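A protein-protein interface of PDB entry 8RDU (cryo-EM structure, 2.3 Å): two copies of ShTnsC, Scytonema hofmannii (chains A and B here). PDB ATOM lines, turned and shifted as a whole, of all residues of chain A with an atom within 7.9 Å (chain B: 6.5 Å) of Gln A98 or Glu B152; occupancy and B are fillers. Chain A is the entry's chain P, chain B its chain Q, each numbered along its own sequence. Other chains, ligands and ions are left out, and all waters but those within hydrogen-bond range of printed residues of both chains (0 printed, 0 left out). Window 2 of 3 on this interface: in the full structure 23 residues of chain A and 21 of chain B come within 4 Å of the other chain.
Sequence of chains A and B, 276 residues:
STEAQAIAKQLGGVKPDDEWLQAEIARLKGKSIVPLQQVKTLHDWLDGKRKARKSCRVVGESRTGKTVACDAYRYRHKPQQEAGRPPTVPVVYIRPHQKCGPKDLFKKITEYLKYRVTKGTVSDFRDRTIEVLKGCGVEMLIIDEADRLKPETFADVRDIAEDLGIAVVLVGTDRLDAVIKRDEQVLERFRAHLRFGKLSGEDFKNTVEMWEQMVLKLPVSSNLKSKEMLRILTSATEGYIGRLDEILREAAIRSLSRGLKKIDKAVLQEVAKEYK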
ATOM      1  N   ARG A  95      -1.330  17.413  -1.573  1.00  0.00           N
ATOM      2  CA  ARG A  95      -2.764  17.575  -1.344  1.00  0.00           C
ATOM      3  C   ARG A  95      -3.475  16.268  -1.629  1.00  0.00           C
ATOM      4  O   ARG A  95      -3.566  15.861  -2.802  1.00  0.00           O
ATOM      5  CB  ARG A  95      -3.341  18.676  -2.229  1.00  0.00           C
ATOM      6  CG  ARG A  95      -4.768  19.046  -1.885  1.00  0.00           C
ATOM      7  CD  ARG A  95      -5.563  19.365  -3.133  1.00  0.00           C
ATOM      8  NE  ARG A  95      -4.873  20.303  -4.007  1.00  0.00           N
ATOM      9  CZ  ARG A  95      -4.864  20.213  -5.329  1.00  0.00           C
ATOM     10  NH1 ARG A  95      -5.649  19.361  -5.968  1.00  0.00           N
ATOM     11  NH2 ARG A  95      -4.087  21.033  -6.029  1.00  0.00           N
ATOM     12  N   PRO A  96      -4.014  15.593  -0.618  1.00  0.00           N
ATOM     13  CA  PRO A  96      -4.764  14.363  -0.867  1.00  0.00           C
ATOM     14  C   PRO A  96      -5.917  14.583  -1.828  1.00  0.00           C
ATOM     15  O   PRO A  96      -6.509  15.659  -1.892  1.00  0.00           O
ATOM     16  CB  PRO A  96      -5.272  13.972   0.527  1.00  0.00           C
ATOM     17  CG  PRO A  96      -4.368  14.652   1.459  1.00  0.00           C
ATOM     18  CD  PRO A  96      -4.010  15.941   0.806  1.00  0.00           C
ATOM     19  N   HIS A  97      -6.220  13.543  -2.594  1.00  0.00           N
ATOM     20  CA  HIS A  97      -7.514  13.445  -3.239  1.00  0.00           C
ATOM     21  C   HIS A  97      -8.589  13.176  -2.192  1.00  0.00           C
ATOM     22  O   HIS A  97      -8.307  12.742  -1.074  1.00  0.00           O
ATOM     23  CB  HIS A  97      -7.496  12.358  -4.310  1.00  0.00           C
ATOM     24  CG  HIS A  97      -6.435  12.558  -5.346  1.00  0.00           C
ATOM     25  ND1 HIS A  97      -6.404  13.658  -6.176  1.00  0.00           N
ATOM     26  CD2 HIS A  97      -5.355  11.810  -5.674  1.00  0.00           C
ATOM     27  CE1 HIS A  97      -5.357  13.574  -6.976  1.00  0.00           C
ATOM     28  NE2 HIS A  97      -4.705  12.462  -6.693  1.00  0.00           N
ATOM     29  N   GLN A  98      -9.833  13.466  -2.555  1.00  0.00           N
ATOM     30  CA  GLN A  98     -10.936  13.278  -1.625  1.00  0.00           C
ATOM     31  C   GLN A  98     -11.055  11.809  -1.226  1.00  0.00           C
ATOM     32  O   GLN A  98     -10.805  10.903  -2.025  1.00  0.00           O
ATOM     33  CB  GLN A  98     -12.243  13.757  -2.263  1.00  0.00           C
ATOM     34  CG  GLN A  98     -13.491  13.712  -1.381  1.00  0.00           C
ATOM     35  CD  GLN A  98     -13.357  14.500  -0.089  1.00  0.00           C
ATOM     36  OE1 GLN A  98     -12.581  14.151   0.800  1.00  0.00           O
ATOM     37  NE2 GLN A  98     -14.119  15.581   0.017  1.00  0.00           N
ATOM     38  N   LYS A  99     -11.450  11.583   0.028  1.00  0.00           N
ATOM     39  CA  LYS A  99     -11.456  10.257   0.652  1.00  0.00           C
ATOM     40  C   LYS A  99     -10.120   9.540   0.472  1.00  0.00           C
ATOM     41  O   LYS A  99     -10.053   8.406  -0.002  1.00  0.00           O
ATOM     42  CB  LYS A  99     -12.606   9.402   0.112  1.00  0.00           C
ATOM     43  CG  LYS A  99     -13.987   9.967   0.389  1.00  0.00           C
ATOM     44  CD  LYS A  99     -14.195  10.177   1.879  1.00  0.00           C
ATOM     45  CE  LYS A  99     -15.610  10.640   2.190  1.00  0.00           C
ATOM     46  NZ  LYS A  99     -16.608   9.547   2.039  1.00  0.00           N
ATOM     47  N   CYS A 100      -9.043  10.221   0.858  1.00  0.00           N
ATOM     48  CA  CYS A 100      -7.706   9.649   0.772  1.00  0.00           C
ATOM     49  C   CYS A 100      -7.546   8.535   1.799  1.00  0.00           C
ATOM     50  O   CYS A 100      -7.575   8.791   3.007  1.00  0.00           O
ATOM     51  CB  CYS A 100      -6.656  10.735   0.985  1.00  0.00           C
ATOM     52  SG  CYS A 100      -4.946  10.156   0.976  1.00  0.00           S
ATOM     53  N   GLY A 101      -7.359   7.307   1.330  1.00  0.00           N
ATOM     54  CA  GLY A 101      -6.984   6.220   2.198  1.00  0.00           C
ATOM     55  C   GLY A 101      -5.490   6.124   2.429  1.00  0.00           C
ATOM     56  O   GLY A 101      -4.707   6.932   1.928  1.00  0.00           O
ATOM     57  N   ASP A 104      -3.502   5.709  -0.846  1.00  0.00           N
ATOM     58  CA  ASP A 104      -3.455   6.981  -1.560  1.00  0.00           C
ATOM     59  C   ASP A 104      -2.438   7.938  -0.952  1.00  0.00           C
ATOM     60  O   ASP A 104      -1.703   8.616  -1.677  1.00  0.00           O
ATOM     61  CB  ASP A 104      -4.843   7.618  -1.559  1.00  0.00           C
ATOM     62  CG  ASP A 104      -5.907   6.691  -2.103  1.00  0.00           C
ATOM     63  OD1 ASP A 104      -5.562   5.784  -2.887  1.00  0.00           O
ATOM     64  OD2 ASP A 104      -7.090   6.859  -1.740  1.00  0.00           O
ATOM     65  N   GLU A 145      -5.539  20.509   2.565  1.00  0.00           N
ATOM     66  CA  GLU A 145      -6.838  19.799   2.538  1.00  0.00           C
ATOM     67  C   GLU A 145      -6.674  18.553   3.404  1.00  0.00           C
ATOM     68  O   GLU A 145      -7.034  17.465   2.945  1.00  0.00           O
ATOM     69  CB  GLU A 145      -7.240  19.487   1.100  1.00  0.00           C
ATOM     70  CG  GLU A 145      -7.168  20.686   0.179  1.00  0.00           C
ATOM     71  CD  GLU A 145      -8.471  21.450   0.040  1.00  0.00           C
ATOM     72  OE1 GLU A 145      -9.525  20.892   0.400  1.00  0.00           O
ATOM     73  OE2 GLU A 145      -8.426  22.600  -0.431  1.00  0.00           O
ATOM     74  N   ALA A 146      -6.163  18.723   4.621  1.00  0.00           N
ATOM     75  CA  ALA A 146      -5.915  17.582   5.537  1.00  0.00           C
ATOM     76  C   ALA A 146      -7.249  16.964   5.947  1.00  0.00           C
ATOM     77  O   ALA A 146      -7.243  15.796   6.349  1.00  0.00           O
ATOM     78  CB  ALA A 146      -5.116  18.050   6.714  1.00  0.00           C
ATOM     79  N   ASP A 147      -8.347  17.711   5.825  1.00  0.00           N
ATOM     80  CA  ASP A 147      -9.678  17.173   6.090  1.00  0.00           C
ATOM     81  C   ASP A 147     -10.135  16.140   5.064  1.00  0.00           C
ATOM     82  O   ASP A 147     -11.147  15.475   5.297  1.00  0.00           O
ATOM     83  CB  ASP A 147     -10.699  18.307   6.159  1.00  0.00           C
ATOM     84  CG  ASP A 147     -10.720  19.149   4.904  1.00  0.00           C
ATOM     85  OD1 ASP A 147      -9.741  19.884   4.667  1.00  0.00           O
ATOM     86  OD2 ASP A 147     -11.715  19.079   4.153  1.00  0.00           O
ATOM     87  N   ARG A 148      -9.440  16.003   3.937  1.00  0.00           N
ATOM     88  CA  ARG A 148      -9.758  14.953   2.978  1.00  0.00           C
ATOM     89  C   ARG A 148      -9.266  13.574   3.403  1.00  0.00           C
ATOM     90  O   ARG A 148      -9.722  12.573   2.839  1.00  0.00           O
ATOM     91  CB  ARG A 148      -9.147  15.293   1.621  1.00  0.00           C
ATOM     92  CG  ARG A 148      -9.760  16.486   0.937  1.00  0.00           C
ATOM     93  CD  ARG A 148      -9.107  16.679  -0.403  1.00  0.00           C
ATOM     94  NE  ARG A 148      -9.666  17.797  -1.149  1.00  0.00           N
ATOM     95  CZ  ARG A 148      -9.341  18.087  -2.400  1.00  0.00           C
ATOM     96  NH1 ARG A 148      -8.451  17.371  -3.064  1.00  0.00           N
ATOM     97  NH2 ARG A 148      -9.912  19.130  -2.992  1.00  0.00           N
ATOM     98  N   LEU A 149      -8.352  13.496   4.367  1.00  0.00           N
ATOM     99  CA  LEU A 149      -7.894  12.205   4.869  1.00  0.00           C
ATOM    100  C   LEU A 149      -9.036  11.437   5.518  1.00  0.00           C
ATOM    101  O   LEU A 149      -9.784  11.982   6.333  1.00  0.00           O
ATOM    102  CB  LEU A 149      -6.752  12.407   5.863  1.00  0.00           C
ATOM    103  CG  LEU A 149      -5.499  13.035   5.270  1.00  0.00           C
ATOM    104  CD1 LEU A 149      -4.449  13.256   6.334  1.00  0.00           C
ATOM    105  CD2 LEU A 149      -4.979  12.139   4.174  1.00  0.00           C
ATOM    106  N   LYS A 150      -9.174  10.165   5.144  1.00  0.00           N
ATOM    107  CA  LYS A 150     -10.087   9.270   5.840  1.00  0.00           C
ATOM    108  C   LYS A 150      -9.718   9.132   7.318  1.00  0.00           C
ATOM    109  O   LYS A 150      -8.540   9.188   7.684  1.00  0.00           O
ATOM    110  CB  LYS A 150     -10.081   7.889   5.191  1.00  0.00           C
ATOM    111  CG  LYS A 150     -10.793   7.795   3.861  1.00  0.00           C
ATOM    112  CD  LYS A 150     -10.860   6.345   3.411  1.00  0.00           C
ATOM    113  CE  LYS A 150     -11.533   6.199   2.062  1.00  0.00           C
ATOM    114  NZ  LYS A 150     -11.630   4.771   1.654  1.00  0.00           N
ATOM    115  N   ARG A 175     -13.411  23.424   8.869  1.00  0.00           N
ATOM    116  CA  ARG A 175     -13.890  22.084   8.542  1.00  0.00           C
ATOM    117  C   ARG A 175     -12.919  21.005   9.009  1.00  0.00           C
ATOM    118  O   ARG A 175     -13.340  19.897   9.358  1.00  0.00           O
ATOM    119  CB  ARG A 175     -14.129  21.997   7.034  1.00  0.00           C
ATOM    120  CG  ARG A 175     -15.066  20.899   6.561  1.00  0.00           C
ATOM    121  CD  ARG A 175     -14.737  20.526   5.124  1.00  0.00           C
ATOM    122  NE  ARG A 175     -15.922  20.273   4.312  1.00  0.00           N
ATOM    123  CZ  ARG A 175     -16.712  19.212   4.415  1.00  0.00           C
ATOM    124  NH1 ARG A 175     -16.535  18.303   5.360  1.00  0.00           N
ATOM    125  NH2 ARG A 175     -17.731  19.080   3.569  1.00  0.00           N
ATOM    126  N   CYS B 100     -24.540  12.065  -8.304  1.00  0.00           N
ATOM    127  CA  CYS B 100     -23.370  11.740  -9.110  1.00  0.00           C
ATOM    128  C   CYS B 100     -22.128  11.619  -8.230  1.00  0.00           C
ATOM    129  O   CYS B 100     -21.732  12.585  -7.571  1.00  0.00           O
ATOM    130  CB  CYS B 100     -23.162  12.807 -10.179  1.00  0.00           C
ATOM    131  SG  CYS B 100     -21.862  12.424 -11.366  1.00  0.00           S
ATOM    132  N   GLY B 101     -21.517  10.439  -8.219  1.00  0.00           N
ATOM    133  CA  GLY B 101     -20.218  10.277  -7.608  1.00  0.00           C
ATOM    134  C   GLY B 101     -19.106  10.700  -8.537  1.00  0.00           C
ATOM    135  O   GLY B 101     -19.310  10.989  -9.723  1.00  0.00           O
ATOM    136  N   PRO B 102     -17.886  10.761  -7.991  1.00  0.00           N
ATOM    137  CA  PRO B 102     -16.732  11.108  -8.839  1.00  0.00           C
ATOM    138  C   PRO B 102     -16.562  10.194 -10.037  1.00  0.00           C
ATOM    139  O   PRO B 102     -16.279  10.675 -11.140  1.00  0.00           O
ATOM    140  CB  PRO B 102     -15.548  11.005  -7.868  1.00  0.00           C
ATOM    141  CG  PRO B 102     -16.146  11.249  -6.530  1.00  0.00           C
ATOM    142  CD  PRO B 102     -17.504  10.607  -6.582  1.00  0.00           C
ATOM    143  N   ARG B 126      -9.991   9.172 -12.424  1.00  0.00           N
ATOM    144  CA  ARG B 126      -9.475  10.529 -12.273  1.00  0.00           C
ATOM    145  C   ARG B 126      -8.320  10.824 -13.228  1.00  0.00           C
ATOM    146  O   ARG B 126      -8.357  11.811 -13.970  1.00  0.00           O
ATOM    147  CB  ARG B 126      -9.055  10.757 -10.824  1.00  0.00           C
ATOM    148  CG  ARG B 126      -8.661  12.181 -10.498  1.00  0.00           C
ATOM    149  CD  ARG B 126      -8.297  12.307  -9.035  1.00  0.00           C
ATOM    150  NE  ARG B 126      -9.461  12.121  -8.181  1.00  0.00           N
ATOM    151  CZ  ARG B 126      -9.664  11.062  -7.412  1.00  0.00           C
ATOM    152  NH1 ARG B 126      -8.748  10.117  -7.286  1.00  0.00           N
ATOM    153  NH2 ARG B 126     -10.804  10.959  -6.734  1.00  0.00           N
ATOM    154  N   LEU B 149     -24.715  16.879  -7.855  1.00  0.00           N
ATOM    155  CA  LEU B 149     -23.454  16.302  -7.395  1.00  0.00           C
ATOM    156  C   LEU B 149     -23.496  15.976  -5.904  1.00  0.00           C
ATOM    157  O   LEU B 149     -24.072  16.720  -5.105  1.00  0.00           O
ATOM    158  CB  LEU B 149     -22.296  17.260  -7.672  1.00  0.00           C
ATOM    159  CG  LEU B 149     -22.011  17.673  -9.114  1.00  0.00           C
ATOM    160  CD1 LEU B 149     -20.893  18.702  -9.136  1.00  0.00           C
ATOM    161  CD2 LEU B 149     -21.656  16.467  -9.965  1.00  0.00           C
ATOM    162  N   LYS B 150     -22.878  14.855  -5.530  1.00  0.00           N
ATOM    163  CA  LYS B 150     -22.665  14.556  -4.120  1.00  0.00           C
ATOM    164  C   LYS B 150     -21.594  15.465  -3.510  1.00  0.00           C
ATOM    165  O   LYS B 150     -20.693  15.939  -4.207  1.00  0.00           O
ATOM    166  CB  LYS B 150     -22.277  13.090  -3.940  1.00  0.00           C
ATOM    167  CG  LYS B 150     -23.403  12.132  -4.292  1.00  0.00           C
ATOM    168  CD  LYS B 150     -23.115  10.716  -3.834  1.00  0.00           C
ATOM    169  CE  LYS B 150     -22.059  10.055  -4.679  1.00  0.00           C
ATOM    170  NZ  LYS B 150     -21.358   8.971  -3.943  1.00  0.00           N
ATOM    171  N   PRO B 151     -21.683  15.725  -2.197  1.00  0.00           N
ATOM    172  CA  PRO B 151     -20.710  16.615  -1.530  1.00  0.00           C
ATOM    173  C   PRO B 151     -19.230  16.273  -1.701  1.00  0.00           C
ATOM    174  O   PRO B 151     -18.411  17.197  -1.782  1.00  0.00           O
ATOM    175  CB  PRO B 151     -21.125  16.520  -0.054  1.00  0.00           C
ATOM    176  CG  PRO B 151     -22.571  16.199  -0.087  1.00  0.00           C
ATOM    177  CD  PRO B 151     -22.764  15.312  -1.285  1.00  0.00           C
ATOM    178  N   GLU B 152     -18.850  14.992  -1.740  1.00  0.00           N
ATOM    179  CA  GLU B 152     -17.449  14.660  -1.995  1.00  0.00           C
ATOM    180  C   GLU B 152     -17.042  14.932  -3.439  1.00  0.00           C
ATOM    181  O   GLU B 152     -15.866  15.203  -3.706  1.00  0.00           O
ATOM    182  CB  GLU B 152     -17.155  13.204  -1.622  1.00  0.00           C
ATOM    183  CG  GLU B 152     -17.656  12.157  -2.601  1.00  0.00           C
ATOM    184  CD  GLU B 152     -19.101  11.778  -2.375  1.00  0.00           C
ATOM    185  OE1 GLU B 152     -19.838  12.567  -1.748  1.00  0.00           O
ATOM    186  OE2 GLU B 152     -19.495  10.679  -2.817  1.00  0.00           O
ATOM    187  N   THR B 153     -17.987  14.863  -4.378  1.00  0.00           N
ATOM    188  CA  THR B 153     -17.660  15.065  -5.786  1.00  0.00           C
ATOM    189  C   THR B 153     -17.234  16.504  -6.066  1.00  0.00           C
ATOM    190  O   THR B 153     -16.437  16.749  -6.976  1.00  0.00           O
ATOM    191  CB  THR B 153     -18.857  14.672  -6.654  1.00  0.00           C
ATOM    192  OG1 THR B 153     -19.306  13.366  -6.274  1.00  0.00           O
ATOM    193  CG2 THR B 153     -18.473  14.638  -8.119  1.00  0.00           C
ATOM    194  N   PHE B 154     -17.753  17.461  -5.292  1.00  0.00           N
ATOM    195  CA  PHE B 154     -17.323  18.855  -5.392  1.00  0.00           C
ATOM    196  C   PHE B 154     -15.832  19.037  -5.134  1.00  0.00           C
ATOM    197  O   PHE B 154     -15.240  20.008  -5.617  1.00  0.00           O
ATOM    198  CB  PHE B 154     -18.132  19.722  -4.433  1.00  0.00           C
ATOM    199  CG  PHE B 154     -19.502  20.048  -4.934  1.00  0.00           C
ATOM    200  CD1 PHE B 154     -19.701  21.126  -5.779  1.00  0.00           C
ATOM    201  CD2 PHE B 154     -20.588  19.277  -4.572  1.00  0.00           C
ATOM    202  CE1 PHE B 154     -20.958  21.431  -6.245  1.00  0.00           C
ATOM    203  CE2 PHE B 154     -21.847  19.578  -5.033  1.00  0.00           C
ATOM    204  CZ  PHE B 154     -22.034  20.655  -5.873  1.00  0.00           C
ATOM    205  N   ALA B 155     -15.209  18.139  -4.373  1.00  0.00           N
ATOM    206  CA  ALA B 155     -13.764  18.222  -4.186  1.00  0.00           C
ATOM    207  C   ALA B 155     -13.013  17.908  -5.473  1.00  0.00           C
ATOM    208  O   ALA B 155     -11.990  18.536  -5.768  1.00  0.00           O
ATOM    209  CB  ALA B 155     -13.323  17.280  -3.068  1.00  0.00           C
ATOM    210  N   ASP B 156     -13.494  16.940  -6.253  1.00  0.00           N
ATOM    211  CA  ASP B 156     -12.922  16.717  -7.577  1.00  0.00           C
ATOM    212  C   ASP B 156     -13.257  17.857  -8.534  1.00  0.00           C
ATOM    213  O   ASP B 156     -12.406  18.286  -9.320  1.00  0.00           O
ATOM    214  CB  ASP B 156     -13.412  15.386  -8.144  1.00  0.00           C
ATOM    215  CG  ASP B 156     -12.654  14.198  -7.591  1.00  0.00           C
ATOM    216  OD1 ASP B 156     -11.407  14.214  -7.631  1.00  0.00           O
ATOM    217  OD2 ASP B 156     -13.304  13.242  -7.125  1.00  0.00           O
ATOM    218  N   VAL B 157     -14.490  18.364  -8.474  1.00  0.00           N
ATOM    219  CA  VAL B 157     -14.889  19.508  -9.291  1.00  0.00           C
ATOM    220  C   VAL B 157     -14.045  20.742  -8.989  1.00  0.00           C
ATOM    221  O   VAL B 157     -13.622  21.458  -9.905  1.00  0.00           O
ATOM    222  CB  VAL B 157     -16.389  19.791  -9.089  1.00  0.00           C
ATOM    223  CG1 VAL B 157     -16.781  21.093  -9.752  1.00  0.00           C
ATOM    224  CG2 VAL B 157     -17.218  18.642  -9.632  1.00  0.00           C
ATOM    225  N   ARG B 158     -13.782  21.012  -7.710  1.00  0.00           N
ATOM    226  CA  ARG B 158     -12.901  22.118  -7.343  1.00  0.00           C
ATOM    227  C   ARG B 158     -11.474  21.925  -7.840  1.00  0.00           C
ATOM    228  O   ARG B 158     -10.838  22.880  -8.300  1.00  0.00           O
ATOM    229  CB  ARG B 158     -12.892  22.292  -5.828  1.00  0.00           C
ATOM    230  CG  ARG B 158     -14.098  22.987  -5.236  1.00  0.00           C
ATOM    231  CD  ARG B 158     -14.045  22.851  -3.731  1.00  0.00           C
ATOM    232  NE  ARG B 158     -12.707  23.130  -3.226  1.00  0.00           N
ATOM    233  CZ  ARG B 158     -12.106  22.436  -2.270  1.00  0.00           C
ATOM    234  NH1 ARG B 158     -12.766  21.554  -1.539  1.00  0.00           N
ATOM    235  NH2 ARG B 158     -10.828  22.675  -2.000  1.00  0.00           N
ATOM    236  N   ASP B 159     -10.943  20.709  -7.738  1.00  0.00           N
ATOM    237  CA  ASP B 159      -9.577  20.470  -8.193  1.00  0.00           C
ATOM    238  C   ASP B 159      -9.456  20.488  -9.711  1.00  0.00           C
ATOM    239  O   ASP B 159      -8.462  20.986 -10.248  1.00  0.00           O
ATOM    240  CB  ASP B 159      -9.074  19.148  -7.620  1.00  0.00           C
ATOM    241  CG  ASP B 159      -8.747  19.250  -6.145  1.00  0.00           C
ATOM    242  OD1 ASP B 159      -9.188  20.231  -5.512  1.00  0.00           O
ATOM    243  OD2 ASP B 159      -8.052  18.355  -5.618  1.00  0.00           O
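NH1 of Arg A95 is in salt-bridge range of OD2 of Asp B159, 2.6 Å away. The guanidinium group of Arg B158 lies within salt-bridge range of the side-chain carboxylate of Glu A145 (2.9 Å). The guanidinium group of Arg A148 lies within salt-bridge range of the side-chain carboxylate of Asp B159 (2.8 Å).
The backbone carbonyl oxygen (O) of Pro A96 lies within hydrogen-bond range of the guanidinium group (NH1) of Arg A148, at 2.8 Å. O of Arg A148 lies within hydrogen-bond range of N of Lys A99, 3.4 Å away. O of Arg A148 is in hydrogen-bond range of N of Cys A100 (3.1 Å). The side-chain carboxylate of Glu A145 is in salt-bridge range of the guanidinium group of Arg A148 (3.5 Å). The guanidinium group of Arg B126 lies within salt-bridge range of the side-chain carboxylate of Asp B156. OE2 of Glu B152 is in salt-bridge range of NZ of Lys B150 (2.8 Å).
His A97 touches Arg B126 (ND1 to CD, 3.7 Å). Glu B152 touches Gln A98. Ala B155 touches Gln A98 (CB to NE2, 3.6 Å). Arg A148 touches Ala B155. Arg B158 touches Arg A148.
Of the printed residues of chain B, Arg A95 touches Asp B159. Of the printed residues of chain B, His A97 touches Arg B126 (3.7 Å). Of the printed residues of chain B, Gln A98 touches Glu B152 (3.6 Å) and Ala B155 (3.6 Å). Of the printed residues of chain B, Glu A145 touches Arg B158 (2.9 Å). Of the printed residues of chain B, Arg A148 touches Ala B155, Arg B158 and Asp B159. Of the printed residues of chain A, Arg B126 touches His A97 (3.7 Å). Lys B150 touches none of the printed residues of chain A. Of the printed residues of chain A, Glu B152 touches Gln A98 (3.6 Å).
Of the 15 printed residues of chain A, 5 touch a printed residue of chain B. Hydrophobic or aromatic side chains of chain A that line the printed part of chain B: His A97. Of the 15 printed residues of chain B, 5 touch a printed residue of chain A. Hydrophobic or aromatic side chains of chain B within 4 Å of the printed part of chain A: Ala B155.
Positions printed for both chains: 100, 101, 149 and 150. Of the 8 pairs that touch across the chains among the printed residues, none has its exchanged pair printed and touching as well.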
